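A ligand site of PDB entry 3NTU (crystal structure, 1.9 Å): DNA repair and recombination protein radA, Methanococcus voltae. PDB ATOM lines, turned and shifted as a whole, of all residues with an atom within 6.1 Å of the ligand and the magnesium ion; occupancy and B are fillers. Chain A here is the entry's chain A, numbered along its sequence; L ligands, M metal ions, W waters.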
ATOM      1  N   GLY A 102     -13.168  35.054  16.611  1.00  0.00           N
ATOM      2  CA  GLY A 102     -13.015  35.322  15.211  1.00  0.00           C
ATOM      3  C   GLY A 102     -14.139  36.185  14.724  1.00  0.00           C
ATOM      4  O   GLY A 102     -15.149  36.337  15.418  1.00  0.00           O
ATOM      5  N   VAL A 103     -13.945  36.768  13.549  1.00  0.00           N
ATOM      6  CA  VAL A 103     -14.958  37.633  12.952  1.00  0.00           C
ATOM      7  C   VAL A 103     -16.184  36.816  12.637  1.00  0.00           C
ATOM      8  O   VAL A 103     -16.151  35.576  12.634  1.00  0.00           O
ATOM      9  CB  VAL A 103     -14.447  38.271  11.631  1.00  0.00           C
ATOM     10  CG1 VAL A 103     -13.272  39.217  11.961  1.00  0.00           C
ATOM     11  CG2 VAL A 103     -13.967  37.191  10.688  1.00  0.00           C
ATOM     12  N   PHE A 104     -17.277  37.496  12.352  1.00  0.00           N
ATOM     13  CA  PHE A 104     -18.521  36.780  12.038  1.00  0.00           C
ATOM     14  C   PHE A 104     -18.328  35.793  10.895  1.00  0.00           C
ATOM     15  O   PHE A 104     -17.560  36.037   9.953  1.00  0.00           O
ATOM     16  CB  PHE A 104     -19.627  37.783  11.627  1.00  0.00           C
ATOM     17  CG  PHE A 104     -19.372  38.471  10.302  1.00  0.00           C
ATOM     18  CD1 PHE A 104     -19.821  37.894   9.115  1.00  0.00           C
ATOM     19  CD2 PHE A 104     -18.639  39.653  10.246  1.00  0.00           C
ATOM     20  CE1 PHE A 104     -19.548  38.472   7.879  1.00  0.00           C
ATOM     21  CE2 PHE A 104     -18.355  40.257   9.003  1.00  0.00           C
ATOM     22  CZ  PHE A 104     -18.805  39.657   7.823  1.00  0.00           C
ATOM     23  N   GLY A 105     -19.042  34.671  10.967  1.00  0.00           N
ATOM     24  CA  GLY A 105     -18.991  33.683   9.905  1.00  0.00           C
ATOM     25  C   GLY A 105     -17.669  32.987   9.684  1.00  0.00           C
ATOM     26  O   GLY A 105     -17.529  32.229   8.717  1.00  0.00           O
ATOM     27  N   SER A 106     -16.705  33.183  10.577  1.00  0.00           N
ATOM     28  CA  SER A 106     -15.418  32.545  10.383  1.00  0.00           C
ATOM     29  C   SER A 106     -15.400  31.042  10.654  1.00  0.00           C
ATOM     30  O   SER A 106     -14.440  30.382  10.277  1.00  0.00           O
ATOM     31  CB  SER A 106     -14.322  33.232  11.218  1.00  0.00           C
ATOM     32  OG  SER A 106     -14.661  33.250  12.599  1.00  0.00           O
ATOM     33  N   GLY A 107     -16.431  30.509  11.314  1.00  0.00           N
ATOM     34  CA  GLY A 107     -16.476  29.060  11.560  1.00  0.00           C
ATOM     35  C   GLY A 107     -16.426  28.597  13.008  1.00  0.00           C
ATOM     36  O   GLY A 107     -16.280  27.427  13.264  1.00  0.00           O
ATOM     37  N   LYS A 108     -16.506  29.532  13.954  1.00  0.00           N
ATOM     38  CA  LYS A 108     -16.476  29.204  15.377  1.00  0.00           C
ATOM     39  C   LYS A 108     -17.527  28.147  15.720  1.00  0.00           C
ATOM     40  O   LYS A 108     -17.215  27.126  16.302  1.00  0.00           O
ATOM     41  CB  LYS A 108     -16.706  30.476  16.260  1.00  0.00           C
ATOM     42  CG  LYS A 108     -15.703  31.596  15.965  1.00  0.00           C
ATOM     43  CD  LYS A 108     -15.939  32.795  16.899  1.00  0.00           C
ATOM     44  CE  LYS A 108     -17.288  33.473  16.595  1.00  0.00           C
ATOM     45  NZ  LYS A 108     -17.250  34.198  15.245  1.00  0.00           N
ATOM     46  N   THR A 109     -18.759  28.426  15.342  1.00  0.00           N
ATOM     47  CA  THR A 109     -19.864  27.486  15.606  1.00  0.00           C
ATOM     48  C   THR A 109     -19.702  26.187  14.822  1.00  0.00           C
ATOM     49  O   THR A 109     -19.998  25.106  15.340  1.00  0.00           O
ATOM     50  CB  THR A 109     -21.236  28.194  15.335  1.00  0.00           C
ATOM     51  OG1 THR A 109     -21.399  29.197  16.349  1.00  0.00           O
ATOM     52  CG2 THR A 109     -22.403  27.181  15.451  1.00  0.00           C
ATOM     53  N   GLN A 110     -19.159  26.265  13.601  1.00  0.00           N
ATOM     54  CA  GLN A 110     -18.943  25.018  12.832  1.00  0.00           C
ATOM     55  C   GLN A 110     -17.922  24.120  13.567  1.00  0.00           C
ATOM     56  O   GLN A 110     -18.080  22.897  13.606  1.00  0.00           O
ATOM     57  CB  GLN A 110     -18.386  25.325  11.445  1.00  0.00           C
ATOM     58  CG  GLN A 110     -19.419  26.103  10.577  1.00  0.00           C
ATOM     59  CD  GLN A 110     -20.715  25.338  10.429  1.00  0.00           C
ATOM     60  OE1 GLN A 110     -20.750  24.279   9.802  1.00  0.00           O
ATOM     61  NE2 GLN A 110     -21.792  25.866  11.002  1.00  0.00           N
ATOM     62  N   ILE A 111     -16.876  24.741  14.133  1.00  0.00           N
ATOM     63  CA  ILE A 111     -15.870  23.937  14.837  1.00  0.00           C
ATOM     64  C   ILE A 111     -16.515  23.270  16.045  1.00  0.00           C
ATOM     65  O   ILE A 111     -16.205  22.116  16.352  1.00  0.00           O
ATOM     66  CB  ILE A 111     -14.657  24.832  15.282  1.00  0.00           C
ATOM     67  CG1 ILE A 111     -13.875  25.237  14.005  1.00  0.00           C
ATOM     68  CG2 ILE A 111     -13.691  24.046  16.280  1.00  0.00           C
ATOM     69  CD1 ILE A 111     -12.892  26.410  14.239  1.00  0.00           C
ATOM     70  N   GLU A 148     -26.690  31.577  21.644  1.00  0.00           N
ATOM     71  CA  GLU A 148     -27.189  32.387  20.536  1.00  0.00           C
ATOM     72  C   GLU A 148     -28.314  31.773  19.719  1.00  0.00           C
ATOM     73  O   GLU A 148     -28.928  32.464  18.891  1.00  0.00           O
ATOM     74  CB  GLU A 148     -26.028  32.752  19.606  1.00  0.00           C
ATOM     75  CG  GLU A 148     -25.000  33.657  20.283  1.00  0.00           C
ATOM     76  CD  GLU A 148     -23.860  34.047  19.345  1.00  0.00           C
ATOM     77  OE1 GLU A 148     -24.029  33.944  18.098  1.00  0.00           O
ATOM     78  OE2 GLU A 148     -22.817  34.490  19.852  1.00  0.00           O
ATOM     79  N   THR A 150     -27.785  29.072  17.766  1.00  0.00           N
ATOM     80  CA  THR A 150     -27.242  28.547  16.521  1.00  0.00           C
ATOM     81  C   THR A 150     -26.921  27.067  16.491  1.00  0.00           C
ATOM     82  O   THR A 150     -26.270  26.593  15.562  1.00  0.00           O
ATOM     83  CB  THR A 150     -25.988  29.341  16.059  1.00  0.00           C
ATOM     84  OG1 THR A 150     -25.212  29.717  17.203  1.00  0.00           O
ATOM     85  CG2 THR A 150     -26.414  30.617  15.303  1.00  0.00           C
ATOM     86  N   ARG A 155     -26.974  20.145  10.816  1.00  0.00           N
ATOM     87  CA  ARG A 155     -25.532  20.247  10.540  1.00  0.00           C
ATOM     88  C   ARG A 155     -24.834  19.059  11.174  1.00  0.00           C
ATOM     89  O   ARG A 155     -23.879  18.484  10.596  1.00  0.00           O
ATOM     90  CB  ARG A 155     -24.935  21.522  11.118  1.00  0.00           C
ATOM     91  CG  ARG A 155     -23.546  21.758  10.616  1.00  0.00           C
ATOM     92  CD  ARG A 155     -23.562  21.813   9.063  1.00  0.00           C
ATOM     93  NE  ARG A 155     -22.297  22.359   8.634  1.00  0.00           N
ATOM     94  CZ  ARG A 155     -21.545  21.876   7.664  1.00  0.00           C
ATOM     95  NH1 ARG A 155     -20.413  22.469   7.413  1.00  0.00           N
ATOM     96  NH2 ARG A 155     -21.944  20.825   6.939  1.00  0.00           N
ATOM     97  N   GLN A 158     -25.301  16.079   8.873  1.00  0.00           N
ATOM     98  CA  GLN A 158     -24.499  16.181   7.674  1.00  0.00           C
ATOM     99  C   GLN A 158     -23.025  15.899   7.960  1.00  0.00           C
ATOM    100  O   GLN A 158     -22.359  15.116   7.250  1.00  0.00           O
ATOM    101  CB  GLN A 158     -24.719  17.573   7.091  1.00  0.00           C
ATOM    102  CG  GLN A 158     -23.978  17.863   5.832  1.00  0.00           C
ATOM    103  CD  GLN A 158     -24.411  19.193   5.253  1.00  0.00           C
ATOM    104  OE1 GLN A 158     -24.697  20.155   5.991  1.00  0.00           O
ATOM    105  NE2 GLN A 158     -24.475  19.269   3.923  1.00  0.00           N
ATOM    106  N   ASP A 208     -21.003  28.253  23.458  1.00  0.00           N
ATOM    107  CA  ASP A 208     -20.997  29.019  22.203  1.00  0.00           C
ATOM    108  C   ASP A 208     -22.218  29.967  22.269  1.00  0.00           C
ATOM    109  O   ASP A 208     -23.343  29.515  22.043  1.00  0.00           O
ATOM    110  CB  ASP A 208     -21.089  27.999  21.017  1.00  0.00           C
ATOM    111  CG  ASP A 208     -21.195  28.678  19.662  1.00  0.00           C
ATOM    112  OD1 ASP A 208     -20.700  29.822  19.482  1.00  0.00           O
ATOM    113  OD2 ASP A 208     -21.775  28.053  18.742  1.00  0.00           O
ATOM    114  N   THR A 252     -16.430  29.799  22.361  1.00  0.00           N
ATOM    115  CA  THR A 252     -16.231  30.694  21.220  1.00  0.00           C
ATOM    116  C   THR A 252     -16.307  32.130  21.747  1.00  0.00           C
ATOM    117  O   THR A 252     -16.884  32.404  22.795  1.00  0.00           O
ATOM    118  CB  THR A 252     -17.312  30.518  20.119  1.00  0.00           C
ATOM    119  OG1 THR A 252     -18.556  30.986  20.636  1.00  0.00           O
ATOM    120  CG2 THR A 252     -17.385  29.098  19.694  1.00  0.00           C
ATOM    121  N   GLN A 254     -16.404  36.525  20.442  1.00  0.00           N
ATOM    122  CA  GLN A 254     -16.555  37.513  19.362  1.00  0.00           C
ATOM    123  C   GLN A 254     -15.360  38.467  19.390  1.00  0.00           C
ATOM    124  O   GLN A 254     -14.488  38.400  20.285  1.00  0.00           O
ATOM    125  CB  GLN A 254     -17.857  38.294  19.571  1.00  0.00           C
ATOM    126  CG  GLN A 254     -19.032  37.345  19.564  1.00  0.00           C
ATOM    127  CD  GLN A 254     -20.374  38.053  19.605  1.00  0.00           C
ATOM    128  OE1 GLN A 254     -20.480  39.154  20.126  1.00  0.00           O
ATOM    129  NE2 GLN A 254     -21.431  37.401  19.085  1.00  0.00           N
ATOM    130  N   ARG A 293     -10.206  28.811   5.537  1.00  0.00           N
ATOM    131  CA  ARG A 293     -10.222  29.493   6.847  1.00  0.00           C
ATOM    132  C   ARG A 293      -8.799  29.457   7.372  1.00  0.00           C
ATOM    133  O   ARG A 293      -7.989  28.639   6.908  1.00  0.00           O
ATOM    134  CB  ARG A 293     -11.147  28.739   7.835  1.00  0.00           C
ATOM    135  CG  ARG A 293     -12.652  28.699   7.414  1.00  0.00           C
ATOM    136  CD  ARG A 293     -13.315  30.073   7.373  1.00  0.00           C
ATOM    137  NE  ARG A 293     -14.740  29.964   6.984  1.00  0.00           N
ATOM    138  CZ  ARG A 293     -15.207  30.098   5.753  1.00  0.00           C
ATOM    139  NH1 ARG A 293     -14.387  30.384   4.715  1.00  0.00           N
ATOM    140  NH2 ARG A 293     -16.494  29.895   5.535  1.00  0.00           N
ATOM    141  N   ILE A 312     -13.948  24.868   5.456  1.00  0.00           N
ATOM    142  CA  ILE A 312     -15.231  24.440   6.018  1.00  0.00           C
ATOM    143  C   ILE A 312     -16.118  24.193   4.777  1.00  0.00           C
ATOM    144  O   ILE A 312     -16.372  25.089   3.970  1.00  0.00           O
ATOM    145  CB  ILE A 312     -15.843  25.502   6.949  1.00  0.00           C
ATOM    146  CG1 ILE A 312     -14.968  25.612   8.205  1.00  0.00           C
ATOM    147  CG2 ILE A 312     -17.263  25.082   7.342  1.00  0.00           C
ATOM    148  CD1 ILE A 312     -15.494  26.609   9.250  1.00  0.00           C
ATOM    149  N   THR A 313     -16.602  22.969   4.637  1.00  0.00           N
ATOM    150  CA  THR A 313     -17.383  22.585   3.452  1.00  0.00           C
ATOM    151  C   THR A 313     -18.636  21.869   3.902  1.00  0.00           C
ATOM    152  O   THR A 313     -18.954  21.851   5.088  1.00  0.00           O
ATOM    153  CB  THR A 313     -16.595  21.587   2.577  1.00  0.00           C
ATOM    154  OG1 THR A 313     -16.387  20.375   3.341  1.00  0.00           O
ATOM    155  CG2 THR A 313     -15.202  22.156   2.201  1.00  0.00           C
ATOM    156  N   GLU A 314     -19.349  21.258   2.953  1.00  0.00           N
ATOM    157  CA  GLU A 314     -20.557  20.547   3.323  1.00  0.00           C
ATOM    158  C   GLU A 314     -20.180  19.405   4.255  1.00  0.00           C
ATOM    159  O   GLU A 314     -20.991  18.953   5.064  1.00  0.00           O
ATOM    160  CB  GLU A 314     -21.318  20.061   2.056  1.00  0.00           C
ATOM    161  CG  GLU A 314     -20.959  18.674   1.503  1.00  0.00           C
ATOM    162  CD  GLU A 314     -19.660  18.645   0.721  1.00  0.00           C
ATOM    163  OE1 GLU A 314     -19.376  17.595   0.084  1.00  0.00           O
ATOM    164  OE2 GLU A 314     -18.919  19.661   0.728  1.00  0.00           O
ATOM    165  N   LYS A 315     -18.931  18.966   4.183  1.00  0.00           N
ATOM    166  CA  LYS A 315     -18.479  17.862   5.038  1.00  0.00           C
ATOM    167  C   LYS A 315     -18.126  18.245   6.466  1.00  0.00           C
ATOM    168  O   LYS A 315     -17.977  17.368   7.316  1.00  0.00           O
ATOM    169  CB  LYS A 315     -17.249  17.192   4.438  1.00  0.00           C
ATOM    170  CG  LYS A 315     -17.414  16.710   3.009  1.00  0.00           C
ATOM    171  CD  LYS A 315     -16.380  15.601   2.755  1.00  0.00           C
ATOM    172  CE  LYS A 315     -16.127  15.431   1.267  1.00  0.00           C
ATOM    173  NZ  LYS A 315     -17.372  15.586   0.494  1.00  0.00           N
HETATM  174  P1  LIG L   1     -20.979  34.084  14.481  1.00  0.00           P
HETATM  175  O1  LIG L   1     -19.921  34.969  14.855  1.00  0.00           O
HETATM  176  O2  LIG L   1     -21.289  33.300  15.695  1.00  0.00           O
HETATM  177  O3  LIG L   1     -21.916  35.074  14.008  1.00  0.00           O
HETATM  178  P2  LIG L   1     -19.471  31.880  13.303  1.00  0.00           P
HETATM  179  O4  LIG L   1     -19.831  31.087  14.506  1.00  0.00           O
HETATM  180  O5  LIG L   1     -18.107  32.250  13.459  1.00  0.00           O
HETATM  181  N1  LIG L   1     -20.235  33.293  13.237  1.00  0.00           N
HETATM  182  P3  LIG L   1     -20.230  29.806  11.643  1.00  0.00           P
HETATM  183  O6  LIG L   1     -19.425  28.746  12.381  1.00  0.00           O
HETATM  184  O7  LIG L   1     -21.647  29.818  12.052  1.00  0.00           O
HETATM  185  O8  LIG L   1     -19.604  31.206  11.873  1.00  0.00           O
HETATM  186  O9  LIG L   1     -20.034  29.512  10.092  1.00  0.00           O
HETATM  187  C1  LIG L   1     -20.988  29.998   9.022  1.00  0.00           C
HETATM  188  C2  LIG L   1     -20.408  29.676   7.838  1.00  0.00           C
HETATM  189  O10 LIG L   1     -20.270  28.196   7.829  1.00  0.00           O
HETATM  190  C3  LIG L   1     -21.421  29.910   6.680  1.00  0.00           C
HETATM  191  O11 LIG L   1     -21.691  31.206   6.408  1.00  0.00           O
HETATM  192  C4  LIG L   1     -21.037  28.838   5.618  1.00  0.00           C
HETATM  193  O12 LIG L   1     -19.836  29.512   4.972  1.00  0.00           O
HETATM  194  C5  LIG L   1     -20.409  27.697   6.458  1.00  0.00           C
HETATM  195  N2  LIG L   1     -21.392  26.689   6.493  1.00  0.00           N
HETATM  196  C6  LIG L   1     -22.390  26.483   7.450  1.00  0.00           C
HETATM  197  N3  LIG L   1     -23.124  25.451   7.120  1.00  0.00           N
HETATM  198  C7  LIG L   1     -22.649  24.955   5.959  1.00  0.00           C
HETATM  199  C8  LIG L   1     -23.029  23.890   5.131  1.00  0.00           C
HETATM  200  N4  LIG L   1     -24.078  23.107   5.442  1.00  0.00           N
HETATM  201  N5  LIG L   1     -22.311  23.652   3.976  1.00  0.00           N
HETATM  202  C9  LIG L   1     -21.208  24.440   3.615  1.00  0.00           C
HETATM  203  N6  LIG L   1     -20.812  25.494   4.401  1.00  0.00           N
HETATM  204  C10 LIG L   1     -21.573  25.704   5.563  1.00  0.00           C
HETATM  205 MG    MG M   1     -21.312  31.310  15.823  1.00  0.00          MG
HETATM  206  O   HOH W   1     -20.703  34.219  18.206  1.00  0.00           O
HETATM  207  O   HOH W   2     -17.293  29.427   8.414  1.00  0.00           O
HETATM  208  O   HOH W   3     -23.256  35.873  16.684  1.00  0.00           O
HETATM  209  O   HOH W   4     -22.984  31.505  17.097  1.00  0.00           O
HETATM  210  O   HOH W   5     -22.441  32.334  11.079  1.00  0.00           O
HETATM  211  O   HOH W   6     -18.816  26.320   3.055  1.00  0.00           O
HETATM  212  O   HOH W   7     -20.041  31.464  17.525  1.00  0.00           O
HETATM  213  O   HOH W   8     -22.754  30.976  14.263  1.00  0.00           O
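The magnesium ion is bound by O4 of the ligand (2.0 Å), O2 of the ligand (2.0 Å), water W4 (2.1 Å), water W7 (2.1 Å), water W8 (2.2 Å) and OG1 of Thr 109 (2.2 Å). The magnesium ion has six donor atoms within binding distance.
O12 of the ligand is in hydrogen-bond range of NH2 of Arg 293 (3.4 Å). The backbone NH (N) of Gly 107 is in hydrogen-bond range of an oxygen (O5) of the ligand (3.2 Å). The backbone NH of Gln 110 lies within hydrogen-bond range of an oxygen (O6) of the ligand (2.8 Å). The backbone NH (N) of Thr 109 is in hydrogen-bond range of an oxygen (O6) of the ligand, at 3.1 Å. An oxygen (O5) of the ligand is in hydrogen-bond range of the backbone NH of Lys 108. N4 of the ligand sits at hydrogen-bond distance from OE1 of Gln 158, 3.1 Å away. NZ of Lys 108 is in salt-bridge range of O5 of the ligand (2.8 Å). The backbone NH (N) of Ser 106 is in hydrogen-bond range of an oxygen (O5) of the ligand, at 3.3 Å.
Water W4 bridges the side-chain carboxylate (OE1) of Glu 148 (2.8 Å) and the side-chain hydroxyl (OG1) of Thr 150 (2.9 Å). Water W7 lies within hydrogen-bond range of OD1 of Asp 208 and OG1 of Thr 252. Water W6 bridges N6 of the ligand (2.5 Å) and O of Ile 312 (2.9 Å). Water W1 bridges OE2 of Glu 148 (2.7 Å) and NE2 of Gln 254 (3.4 Å). Water W3 lies within hydrogen-bond range of OE1 of Glu 148 (2.5 Å), O3 of the ligand (3.1 Å) and NE2 of Gln 254 (3.4 Å). Water W2 lies within hydrogen-bond range of O of Gly 105, NE of Arg 293, N of Gly 107 and O9 of the ligand.
The backbone NH (N) of Gly 105 sits close to a nitrogen (N1) of the ligand, 2.9 Å away. The guanidinium group (NH2) of Arg 155 sits close to a nitrogen (N4) of the ligand. Merely in contact with the ligand: Glu 314, Phe 104, Thr 313, Glu 148 and Val 103. Of the 22 residues printed, 14 come within 4 Å of the ligand.
Merely in contact with the magnesium ion: Asp 208 (3.997 Å). Of the 22 residues printed, 2 come within 4 Å of the magnesium ion. Along chain A the residues within 4 Å of the magnesium ion span positions 109 to 208. The nearest printed residue that does not touch the magnesium ion is Glu 148 (4.4 Å).
The side-chain amino group (NZ) of Lys 108 is in hydrogen-bond range of the backbone carbonyl oxygen (O) of Val 103, 3.2 Å away. O of Glu 314 sits at hydrogen-bond distance from NH2 of Arg 155. NZ of Lys 108 sits at hydrogen-bond distance from O of Gly 102. The side-chain amide oxygen (OE1) of Gln 110 sits at hydrogen-bond distance from the guanidinium group (NE) of Arg 155, at 2.7 Å. OD2 of Asp 208 lies close to OG1 of Thr 109 (2.7 Å). The side-chain hydroxyl of Ser 106 sits at hydrogen-bond distance from the backbone carbonyl oxygen of Val 103 (2.8 Å). O of Ser 106 sits close to NE of Arg 293, 3.3 Å away. The side-chain hydroxyl of Thr 252 is in hydrogen-bond range of the side-chain carboxylate of Asp 208.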
